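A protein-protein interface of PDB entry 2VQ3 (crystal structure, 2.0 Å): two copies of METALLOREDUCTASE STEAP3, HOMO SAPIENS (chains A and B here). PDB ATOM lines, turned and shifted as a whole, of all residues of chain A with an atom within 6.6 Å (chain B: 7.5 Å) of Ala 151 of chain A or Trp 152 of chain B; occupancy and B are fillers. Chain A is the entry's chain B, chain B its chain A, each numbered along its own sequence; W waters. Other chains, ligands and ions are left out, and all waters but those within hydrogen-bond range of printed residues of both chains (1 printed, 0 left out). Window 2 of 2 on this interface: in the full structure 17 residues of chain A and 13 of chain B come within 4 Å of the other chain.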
ATOM      1  N   ASP A  38     -22.714 -17.688  16.536  1.00  0.00           N
ATOM      2  CA  ASP A  38     -22.149 -17.629  17.879  1.00  0.00           C
ATOM      3  C   ASP A  38     -20.655 -17.906  17.881  1.00  0.00           C
ATOM      4  O   ASP A  38     -19.902 -17.232  18.580  1.00  0.00           O
ATOM      5  CB  ASP A  38     -22.835 -18.630  18.825  1.00  0.00           C
ATOM      6  CG  ASP A  38     -24.237 -18.221  19.206  1.00  0.00           C
ATOM      7  OD1 ASP A  38     -24.624 -17.052  18.967  1.00  0.00           O
ATOM      8  OD2 ASP A  38     -24.954 -19.082  19.770  1.00  0.00           O
ATOM      9  N   PHE A  39     -20.220 -18.909  17.124  1.00  0.00           N
ATOM     10  CA  PHE A  39     -18.790 -19.218  17.085  1.00  0.00           C
ATOM     11  C   PHE A  39     -17.960 -18.135  16.387  1.00  0.00           C
ATOM     12  O   PHE A  39     -16.936 -17.698  16.944  1.00  0.00           O
ATOM     13  CB  PHE A  39     -18.523 -20.582  16.485  1.00  0.00           C
ATOM     14  CG  PHE A  39     -17.194 -21.171  16.911  1.00  0.00           C
ATOM     15  CD1 PHE A  39     -17.072 -21.796  18.130  1.00  0.00           C
ATOM     16  CD2 PHE A  39     -16.088 -21.084  16.102  1.00  0.00           C
ATOM     17  CE1 PHE A  39     -15.860 -22.354  18.530  1.00  0.00           C
ATOM     18  CE2 PHE A  39     -14.867 -21.644  16.502  1.00  0.00           C
ATOM     19  CZ  PHE A  39     -14.766 -22.271  17.710  1.00  0.00           C
ATOM     20  N   ARG A  41     -18.651 -15.128  16.265  1.00  0.00           N
ATOM     21  CA  ARG A  41     -18.703 -13.879  16.985  1.00  0.00           C
ATOM     22  C   ARG A  41     -17.762 -14.024  18.213  1.00  0.00           C
ATOM     23  O   ARG A  41     -17.100 -13.090  18.612  1.00  0.00           O
ATOM     24  CB  ARG A  41     -20.132 -13.554  17.411  1.00  0.00           C
ATOM     25  CG  ARG A  41     -20.288 -12.256  18.148  1.00  0.00           C
ATOM     26  CD  ARG A  41     -21.745 -11.954  18.521  1.00  0.00           C
ATOM     27  NE  ARG A  41     -22.148 -12.638  19.743  1.00  0.00           N
ATOM     28  CZ  ARG A  41     -22.936 -13.692  19.747  1.00  0.00           C
ATOM     29  NH1 ARG A  41     -23.416 -14.139  18.608  1.00  0.00           N
ATOM     30  NH2 ARG A  41     -23.271 -14.286  20.872  1.00  0.00           N
ATOM     31  N   SER A  42     -17.722 -15.219  18.789  1.00  0.00           N
ATOM     32  CA  SER A  42     -16.859 -15.490  19.921  1.00  0.00           C
ATOM     33  C   SER A  42     -15.375 -15.500  19.528  1.00  0.00           C
ATOM     34  O   SER A  42     -14.569 -14.927  20.227  1.00  0.00           O
ATOM     35  CB  SER A  42     -17.309 -16.752  20.657  1.00  0.00           C
ATOM     36  OG  SER A  42     -18.669 -16.666  21.037  1.00  0.00           O
ATOM     37  N   LEU A  43     -15.032 -16.119  18.398  1.00  0.00           N
ATOM     38  CA  LEU A  43     -13.713 -16.083  17.781  1.00  0.00           C
ATOM     39  C   LEU A  43     -13.261 -14.635  17.550  1.00  0.00           C
ATOM     40  O   LEU A  43     -12.172 -14.265  17.876  1.00  0.00           O
ATOM     41  CB  LEU A  43     -13.701 -16.774  16.408  1.00  0.00           C
ATOM     42  CG  LEU A  43     -13.475 -18.283  16.299  1.00  0.00           C
ATOM     43  CD1 LEU A  43     -13.710 -18.704  14.850  1.00  0.00           C
ATOM     44  CD2 LEU A  43     -12.073 -18.668  16.759  1.00  0.00           C
ATOM     45  N   ILE A 149     -13.136 -26.437  21.534  1.00  0.00           N
ATOM     46  CA  ILE A 149     -13.278 -25.257  22.397  1.00  0.00           C
ATOM     47  C   ILE A 149     -14.696 -24.693  22.258  1.00  0.00           C
ATOM     48  O   ILE A 149     -15.136 -24.407  21.147  1.00  0.00           O
ATOM     49  CB  ILE A 149     -12.274 -24.137  21.997  1.00  0.00           C
ATOM     50  CG1 ILE A 149     -10.817 -24.634  22.032  1.00  0.00           C
ATOM     51  CG2 ILE A 149     -12.418 -22.902  22.919  1.00  0.00           C
ATOM     52  CD1 ILE A 149     -10.356 -25.307  23.335  1.00  0.00           C
ATOM     53  N   SER A 150     -15.402 -24.498  23.368  1.00  0.00           N
ATOM     54  CA  SER A 150     -16.732 -23.870  23.320  1.00  0.00           C
ATOM     55  C   SER A 150     -16.646 -22.376  22.973  1.00  0.00           C
ATOM     56  O   SER A 150     -15.637 -21.722  23.216  1.00  0.00           O
ATOM     57  CB  SER A 150     -17.495 -24.055  24.636  1.00  0.00           C
ATOM     58  OG  SER A 150     -17.038 -23.165  25.656  1.00  0.00           O
ATOM     59  N   ALA A 151     -17.726 -21.858  22.407  1.00  0.00           N
ATOM     60  CA  ALA A 151     -17.851 -20.442  22.097  1.00  0.00           C
ATOM     61  C   ALA A 151     -17.694 -19.605  23.362  1.00  0.00           C
ATOM     62  O   ALA A 151     -17.025 -18.585  23.340  1.00  0.00           O
ATOM     63  CB  ALA A 151     -19.185 -20.160  21.412  1.00  0.00           C
ATOM     64  N   TRP A 152     -18.274 -20.041  24.481  1.00  0.00           N
ATOM     65  CA  TRP A 152     -18.098 -19.280  25.723  1.00  0.00           C
ATOM     66  C   TRP A 152     -16.660 -19.302  26.241  1.00  0.00           C
ATOM     67  O   TRP A 152     -16.203 -18.324  26.828  1.00  0.00           O
ATOM     68  CB  TRP A 152     -19.084 -19.697  26.822  1.00  0.00           C
ATOM     69  CG  TRP A 152     -18.924 -18.814  28.053  1.00  0.00           C
ATOM     70  CD1 TRP A 152     -18.529 -19.204  29.299  1.00  0.00           C
ATOM     71  CD2 TRP A 152     -19.127 -17.391  28.123  1.00  0.00           C
ATOM     72  NE1 TRP A 152     -18.500 -18.115  30.145  1.00  0.00           N
ATOM     73  CE2 TRP A 152     -18.853 -16.993  29.439  1.00  0.00           C
ATOM     74  CE3 TRP A 152     -19.523 -16.419  27.197  1.00  0.00           C
ATOM     75  CZ2 TRP A 152     -18.953 -15.665  29.850  1.00  0.00           C
ATOM     76  CZ3 TRP A 152     -19.639 -15.099  27.615  1.00  0.00           C
ATOM     77  CH2 TRP A 152     -19.339 -14.734  28.922  1.00  0.00           C
ATOM     78  N   THR A 153     -15.949 -20.388  26.028  1.00  0.00           N
ATOM     79  CA  THR A 153     -14.538 -20.450  26.404  1.00  0.00           C
ATOM     80  C   THR A 153     -13.719 -19.463  25.583  1.00  0.00           C
ATOM     81  O   THR A 153     -12.854 -18.788  26.099  1.00  0.00           O
ATOM     82  CB  THR A 153     -13.990 -21.856  26.250  1.00  0.00           C
ATOM     83  OG1 THR A 153     -14.640 -22.692  27.199  1.00  0.00           O
ATOM     84  CG2 THR A 153     -12.506 -21.899  26.479  1.00  0.00           C
ATOM     85  N   LEU A 154     -14.028 -19.376  24.299  1.00  0.00           N
ATOM     86  CA  LEU A 154     -13.440 -18.373  23.448  1.00  0.00           C
ATOM     87  C   LEU A 154     -13.715 -16.978  23.968  1.00  0.00           C
ATOM     88  O   LEU A 154     -12.809 -16.202  24.107  1.00  0.00           O
ATOM     89  CB  LEU A 154     -13.935 -18.510  22.011  1.00  0.00           C
ATOM     90  CG  LEU A 154     -13.167 -19.466  21.124  1.00  0.00           C
ATOM     91  CD1 LEU A 154     -13.903 -19.610  19.831  1.00  0.00           C
ATOM     92  CD2 LEU A 154     -11.745 -19.017  20.893  1.00  0.00           C
ATOM     93  N   GLN A 155     -14.960 -16.675  24.269  1.00  0.00           N
ATOM     94  CA  GLN A 155     -15.342 -15.370  24.788  1.00  0.00           C
ATOM     95  C   GLN A 155     -14.647 -15.051  26.096  1.00  0.00           C
ATOM     96  O   GLN A 155     -13.944 -14.073  26.196  1.00  0.00           O
ATOM     97  CB  GLN A 155     -16.828 -15.339  25.085  1.00  0.00           C
ATOM     98  CG  GLN A 155     -17.695 -15.474  23.912  1.00  0.00           C
ATOM     99  CD  GLN A 155     -18.425 -14.218  23.604  1.00  0.00           C
ATOM    100  OE1 GLN A 155     -18.355 -13.259  24.340  1.00  0.00           O
ATOM    101  NE2 GLN A 155     -19.110 -14.215  22.503  1.00  0.00           N
ATOM    102  N   ALA A 156     -14.900 -15.874  27.095  1.00  0.00           N
ATOM    103  CA  ALA A 156     -14.554 -15.556  28.465  1.00  0.00           C
ATOM    104  C   ALA A 156     -13.256 -16.169  28.882  1.00  0.00           C
ATOM    105  O   ALA A 156     -12.501 -15.595  29.644  1.00  0.00           O
ATOM    106  CB  ALA A 156     -15.601 -16.060  29.350  1.00  0.00           C
ATOM    107  N   GLY A 157     -13.040 -17.364  28.366  1.00  0.00           N
ATOM    108  CA  GLY A 157     -12.203 -18.362  28.991  1.00  0.00           C
ATOM    109  C   GLY A 157     -10.839 -17.908  29.326  1.00  0.00           C
ATOM    110  O   GLY A 157     -10.296 -17.206  28.561  1.00  0.00           O
ATOM    111  N   LEU A 206     -16.386 -31.949  22.880  1.00  0.00           N
ATOM    112  CA  LEU A 206     -16.334 -30.542  23.151  1.00  0.00           C
ATOM    113  C   LEU A 206     -16.261 -30.346  24.650  1.00  0.00           C
ATOM    114  O   LEU A 206     -16.964 -30.995  25.413  1.00  0.00           O
ATOM    115  CB  LEU A 206     -17.547 -29.830  22.566  1.00  0.00           C
ATOM    116  CG  LEU A 206     -17.650 -28.313  22.755  1.00  0.00           C
ATOM    117  CD1 LEU A 206     -16.711 -27.607  21.849  1.00  0.00           C
ATOM    118  CD2 LEU A 206     -19.050 -27.849  22.460  1.00  0.00           C
ATOM    119  N   ARG A 207     -15.376 -29.437  25.025  1.00  0.00           N
ATOM    120  CA  ARG A 207     -15.147 -29.012  26.388  1.00  0.00           C
ATOM    121  C   ARG A 207     -15.726 -27.613  26.614  1.00  0.00           C
ATOM    122  O   ARG A 207     -15.376 -26.667  25.924  1.00  0.00           O
ATOM    123  CB  ARG A 207     -13.651 -28.951  26.653  1.00  0.00           C
ATOM    124  CG  ARG A 207     -12.905 -30.196  26.264  1.00  0.00           C
ATOM    125  CD  ARG A 207     -13.008 -31.289  27.320  1.00  0.00           C
ATOM    126  NE  ARG A 207     -12.281 -32.465  26.864  1.00  0.00           N
ATOM    127  CZ  ARG A 207     -12.275 -33.642  27.475  1.00  0.00           C
ATOM    128  NH1 ARG A 207     -12.952 -33.818  28.599  1.00  0.00           N
ATOM    129  NH2 ARG A 207     -11.568 -34.642  26.964  1.00  0.00           N
ATOM    130  N   ASP B  38     -17.819  -9.141  31.314  1.00  0.00           N
ATOM    131  CA  ASP B  38     -18.476 -10.213  30.568  1.00  0.00           C
ATOM    132  C   ASP B  38     -19.986 -10.104  30.630  1.00  0.00           C
ATOM    133  O   ASP B  38     -20.684 -10.288  29.626  1.00  0.00           O
ATOM    134  CB  ASP B  38     -18.019 -11.589  31.067  1.00  0.00           C
ATOM    135  CG  ASP B  38     -16.601 -11.954  30.596  1.00  0.00           C
ATOM    136  OD1 ASP B  38     -16.122 -11.417  29.577  1.00  0.00           O
ATOM    137  OD2 ASP B  38     -15.955 -12.792  31.250  1.00  0.00           O
ATOM    138  N   PHE B  39     -20.503  -9.792  31.807  1.00  0.00           N
ATOM    139  CA  PHE B  39     -21.950  -9.635  31.960  1.00  0.00           C
ATOM    140  C   PHE B  39     -22.507  -8.406  31.241  1.00  0.00           C
ATOM    141  O   PHE B  39     -23.503  -8.528  30.509  1.00  0.00           O
ATOM    142  CB  PHE B  39     -22.353  -9.628  33.418  1.00  0.00           C
ATOM    143  CG  PHE B  39     -23.799  -9.984  33.621  1.00  0.00           C
ATOM    144  CD1 PHE B  39     -24.209 -11.298  33.582  1.00  0.00           C
ATOM    145  CD2 PHE B  39     -24.747  -9.007  33.821  1.00  0.00           C
ATOM    146  CE1 PHE B  39     -25.533 -11.630  33.752  1.00  0.00           C
ATOM    147  CE2 PHE B  39     -26.095  -9.369  34.007  1.00  0.00           C
ATOM    148  CZ  PHE B  39     -26.460 -10.652  33.963  1.00  0.00           C
ATOM    149  N   SER B  42     -22.515  -9.121  27.540  1.00  0.00           N
ATOM    150  CA  SER B  42     -23.537 -10.110  27.194  1.00  0.00           C
ATOM    151  C   SER B  42     -24.944  -9.523  27.263  1.00  0.00           C
ATOM    152  O   SER B  42     -25.727  -9.708  26.368  1.00  0.00           O
ATOM    153  CB  SER B  42     -23.405 -11.335  28.068  1.00  0.00           C
ATOM    154  OG  SER B  42     -22.160 -11.925  27.867  1.00  0.00           O
ATOM    155  N   ILE B 149     -29.148 -15.763  35.653  1.00  0.00           N
ATOM    156  CA  ILE B 149     -28.915 -15.986  34.225  1.00  0.00           C
ATOM    157  C   ILE B 149     -27.427 -15.837  33.906  1.00  0.00           C
ATOM    158  O   ILE B 149     -26.830 -14.806  34.221  1.00  0.00           O
ATOM    159  CB  ILE B 149     -29.722 -14.973  33.378  1.00  0.00           C
ATOM    160  CG1 ILE B 149     -31.219 -15.002  33.742  1.00  0.00           C
ATOM    161  CG2 ILE B 149     -29.547 -15.269  31.887  1.00  0.00           C
ATOM    162  CD1 ILE B 149     -31.897 -16.376  33.540  1.00  0.00           C
ATOM    163  N   SER B 150     -26.826 -16.856  33.296  1.00  0.00           N
ATOM    164  CA  SER B 150     -25.402 -16.795  32.912  1.00  0.00           C
ATOM    165  C   SER B 150     -25.191 -15.833  31.766  1.00  0.00           C
ATOM    166  O   SER B 150     -26.099 -15.627  30.954  1.00  0.00           O
ATOM    167  CB  SER B 150     -24.884 -18.159  32.487  1.00  0.00           C
ATOM    168  OG  SER B 150     -25.451 -18.564  31.244  1.00  0.00           O
ATOM    169  N   ALA B 151     -23.977 -15.285  31.691  1.00  0.00           N
ATOM    170  CA  ALA B 151     -23.561 -14.421  30.596  1.00  0.00           C
ATOM    171  C   ALA B 151     -23.739 -15.148  29.264  1.00  0.00           C
ATOM    172  O   ALA B 151     -24.201 -14.564  28.285  1.00  0.00           O
ATOM    173  CB  ALA B 151     -22.091 -13.976  30.783  1.00  0.00           C
ATOM    174  N   TRP B 152     -23.394 -16.425  29.204  1.00  0.00           N
ATOM    175  CA  TRP B 152     -23.583 -17.158  27.937  1.00  0.00           C
ATOM    176  C   TRP B 152     -25.049 -17.309  27.573  1.00  0.00           C
ATOM    177  O   TRP B 152     -25.414 -17.265  26.390  1.00  0.00           O
ATOM    178  CB  TRP B 152     -22.911 -18.533  27.936  1.00  0.00           C
ATOM    179  CG  TRP B 152     -23.041 -19.183  26.554  1.00  0.00           C
ATOM    180  CD1 TRP B 152     -23.719 -20.321  26.241  1.00  0.00           C
ATOM    181  CD2 TRP B 152     -22.529 -18.669  25.319  1.00  0.00           C
ATOM    182  NE1 TRP B 152     -23.630 -20.572  24.885  1.00  0.00           N
ATOM    183  CE2 TRP B 152     -22.917 -19.563  24.298  1.00  0.00           C
ATOM    184  CE3 TRP B 152     -21.782 -17.536  24.974  1.00  0.00           C
ATOM    185  CZ2 TRP B 152     -22.580 -19.360  22.964  1.00  0.00           C
ATOM    186  CZ3 TRP B 152     -21.439 -17.341  23.639  1.00  0.00           C
ATOM    187  CH2 TRP B 152     -21.848 -18.245  22.654  1.00  0.00           C
ATOM    188  N   THR B 153     -25.905 -17.495  28.569  1.00  0.00           N
ATOM    189  CA  THR B 153     -27.349 -17.588  28.289  1.00  0.00           C
ATOM    190  C   THR B 153     -27.848 -16.288  27.702  1.00  0.00           C
ATOM    191  O   THR B 153     -28.634 -16.295  26.763  1.00  0.00           O
ATOM    192  CB  THR B 153     -28.194 -17.918  29.532  1.00  0.00           C
ATOM    193  OG1 THR B 153     -27.857 -19.215  29.975  1.00  0.00           O
ATOM    194  CG2 THR B 153     -29.707 -17.892  29.213  1.00  0.00           C
ATOM    195  N   LEU B 154     -27.391 -15.174  28.248  1.00  0.00           N
ATOM    196  CA  LEU B 154     -27.610 -13.870  27.625  1.00  0.00           C
ATOM    197  C   LEU B 154     -27.150 -13.797  26.172  1.00  0.00           C
ATOM    198  O   LEU B 154     -27.911 -13.390  25.315  1.00  0.00           O
ATOM    199  CB  LEU B 154     -26.980 -12.753  28.431  1.00  0.00           C
ATOM    200  CG  LEU B 154     -27.835 -12.299  29.608  1.00  0.00           C
ATOM    201  CD1 LEU B 154     -27.112 -11.298  30.440  1.00  0.00           C
ATOM    202  CD2 LEU B 154     -29.132 -11.736  29.115  1.00  0.00           C
ATOM    203  N   GLN B 155     -25.922 -14.210  25.902  1.00  0.00           N
ATOM    204  CA  GLN B 155     -25.341 -14.173  24.573  1.00  0.00           C
ATOM    205  C   GLN B 155     -26.062 -15.073  23.582  1.00  0.00           C
ATOM    206  O   GLN B 155     -26.449 -14.635  22.522  1.00  0.00           O
ATOM    207  CB  GLN B 155     -23.902 -14.658  24.606  1.00  0.00           C
ATOM    208  CG  GLN B 155     -22.954 -13.791  25.334  1.00  0.00           C
ATOM    209  CD  GLN B 155     -22.068 -13.073  24.426  1.00  0.00           C
ATOM    210  OE1 GLN B 155     -22.101 -13.293  23.243  1.00  0.00           O
ATOM    211  NE2 GLN B 155     -21.259 -12.201  24.966  1.00  0.00           N
ATOM    212  N   ALA B 156     -26.186 -16.339  23.936  1.00  0.00           N
ATOM    213  CA  ALA B 156     -26.659 -17.364  23.035  1.00  0.00           C
ATOM    214  C   ALA B 156     -28.142 -17.228  22.870  1.00  0.00           C
ATOM    215  O   ALA B 156     -28.729 -17.794  21.970  1.00  0.00           O
ATOM    216  CB  ALA B 156     -26.313 -18.715  23.542  1.00  0.00           C
ATOM    217  N   GLY B 157     -28.755 -16.581  23.841  1.00  0.00           N
ATOM    218  CA  GLY B 157     -30.192 -16.562  23.939  1.00  0.00           C
ATOM    219  C   GLY B 157     -30.840 -17.593  24.775  1.00  0.00           C
ATOM    220  O   GLY B 157     -30.469 -18.705  24.703  1.00  0.00           O
ATOM    221  N   PRO B 158     -31.848 -17.212  25.549  1.00  0.00           N
ATOM    222  CA  PRO B 158     -32.577 -18.200  26.326  1.00  0.00           C
ATOM    223  C   PRO B 158     -33.274 -19.208  25.417  1.00  0.00           C
ATOM    224  O   PRO B 158     -33.664 -18.875  24.297  1.00  0.00           O
ATOM    225  CB  PRO B 158     -33.623 -17.375  27.054  1.00  0.00           C
ATOM    226  CG  PRO B 158     -33.760 -16.155  26.292  1.00  0.00           C
ATOM    227  CD  PRO B 158     -32.477 -15.889  25.599  1.00  0.00           C
ATOM    228  N   ARG B 207     -27.780 -20.532  36.836  1.00  0.00           N
ATOM    229  CA  ARG B 207     -28.091 -21.578  35.877  1.00  0.00           C
ATOM    230  C   ARG B 207     -27.224 -21.493  34.618  1.00  0.00           C
ATOM    231  O   ARG B 207     -27.124 -20.434  34.014  1.00  0.00           O
ATOM    232  CB  ARG B 207     -29.548 -21.444  35.527  1.00  0.00           C
ATOM    233  CG  ARG B 207     -30.113 -22.611  34.804  1.00  0.00           C
ATOM    234  CD  ARG B 207     -31.374 -22.200  34.090  1.00  0.00           C
ATOM    235  NE  ARG B 207     -31.189 -21.075  33.170  1.00  0.00           N
ATOM    236  CZ  ARG B 207     -31.859 -19.938  33.213  1.00  0.00           C
ATOM    237  NH1 ARG B 207     -32.807 -19.693  34.131  1.00  0.00           N
ATOM    238  NH2 ARG B 207     -31.598 -19.058  32.308  1.00  0.00           N
ATOM    239  N   LEU B 208     -26.667 -22.635  34.203  1.00  0.00           N
ATOM    240  CA  LEU B 208     -26.041 -22.801  32.853  1.00  0.00           C
ATOM    241  C   LEU B 208     -26.855 -23.449  31.706  1.00  0.00           C
ATOM    242  O   LEU B 208     -27.507 -22.745  30.968  1.00  0.00           O
ATOM    243  CB  LEU B 208     -24.661 -23.442  33.015  1.00  0.00           C
ATOM    244  CG  LEU B 208     -23.795 -22.522  33.892  1.00  0.00           C
ATOM    245  CD1 LEU B 208     -22.466 -23.088  34.281  1.00  0.00           C
ATOM    246  CD2 LEU B 208     -23.645 -21.133  33.339  1.00  0.00           C
ATOM    247  N   LEU B 209     -26.759 -24.759  31.489  1.00  0.00           N
ATOM    248  CA  LEU B 209     -26.943 -25.319  30.130  1.00  0.00           C
ATOM    249  C   LEU B 209     -28.357 -25.855  29.870  1.00  0.00           C
ATOM    250  O   LEU B 209     -28.844 -25.899  28.737  1.00  0.00           O
ATOM    251  CB  LEU B 209     -25.909 -26.383  29.843  1.00  0.00           C
HETATM  252  O   HOH W   1     -21.742 -17.965  30.869  1.00  0.00           O
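Of the printed residues of chain B, Asp 38 of chain A touches Trp 152 (3.97 Å). Of the printed residues of chain B, Ser 42 of chain A touches Trp 152 (3.9 Å). Ala 151 of chain A touches just one residue of chain B: Trp 152 (3.5 Å). Ser 150 of chain B touches none of the printed residues of chain A. Printed residues of chain A within 4 Å of Ala 151 of chain B: Trp 152 (3.4 Å). Trp 152 of chain B touches four residues of chain A. The nearest residue of chain A that does not touch Trp 152 of chain B is Gln 155 of chain A (4.1 Å). The nearest printed residue of chain B that does not touch Ala 156 of chain A is Ala 151 of chain B (7.0 Å).
Water W1 bridges the backbone NH (N) of Trp 152 of chain B (2.8 Å) and the indole nitrogen (NE1) of Trp 152 of chain A (3.3 Å).
The guanidinium group of Arg 41 of chain A is in salt-bridge range of the side-chain carboxylate of Asp 38 of chain A (3.2 Å). The side-chain hydroxyl of Ser 42 of chain A lies close to the backbone carbonyl oxygen of Ala 151 of chain A (3.4 Å). The side-chain hydroxyl (OG) of Ser 42 of chain B sits close to the backbone carbonyl oxygen (O) of Ala 151 of chain B, at 3.4 Å. O of Asp 38 of chain B lies within hydrogen-bond range of OG of Ser 42 of chain B, at 2.8 Å. The side-chain hydroxyl (OG) of Ser 42 of chain B lies within hydrogen-bond range of the side-chain amide nitrogen (NE2) of Gln 155 of chain B (3.1 Å). The side-chain hydroxyl (OG) of Ser 42 of chain A lies within hydrogen-bond range of the backbone carbonyl oxygen (O) of Asp 38 of chain A, 2.8 Å away.
OE1 of Gln 155 of chain B is in hydrogen-bond range of NH2 of Arg 41 of chain A, at 2.8 Å. The side-chain amide nitrogen (NE2) of Gln 155 of chain B lies within hydrogen-bond range of the side-chain amide oxygen (OE1) of Gln 155 of chain A, 3.2 Å away.
Among the printed residues, merely in contact across the chains: Trp 152 of chain A with Trp 152 of chain B (3.4 Å), Trp 152 of chain A with Ala 151 of chain B (3.4 Å), Ala 151 of chain A with Trp 152 of chain B (3.5 Å), Ala 156 of chain A with Asp 38 of chain B (3.8 Å), Ser 42 of chain A with Trp 152 of chain B (3.9 Å) and Asp 38 of chain A with Trp 152 of chain B (3.97 Å).
Asp 38 of chain A touches Trp 152 of chain B, but with the chains exchanged Trp 152 of chain A does not touch Asp 38 of chain B (4.03 Å). Ser 42 of chain A touches Trp 152 of chain B, but with the chains exchanged Trp 152 of chain A does not touch Ser 42 of chain B (4.1 Å). Trp 152 of chain A touches its own counterpart, Trp 152 of chain B. Ala 156 of chain A touches Asp 38 of chain B, but with the chains exchanged Asp 38 of chain A does not touch Ala 156 of chain B (4.03 Å). 13 positions are printed for both chains. Of the 8 pairs that touch across the chains among the printed residues, 4 have their exchanged pair printed and touching as well.
Hydrophobic or aromatic side chains of chain A within 4 Å of the printed part of chain B: Ala 151, Trp 152 and Ala 156. Hydrophobic or aromatic side chains of chain B within 4 Å of the printed part of chain A: Ala 151 and Trp 152. Among the printed residues, 8 pairs touch across the chains. Among the printed residues, no Asp or Glu carboxylate lies within 4 Å of a Lys or Arg side-chain nitrogen of the other chain.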
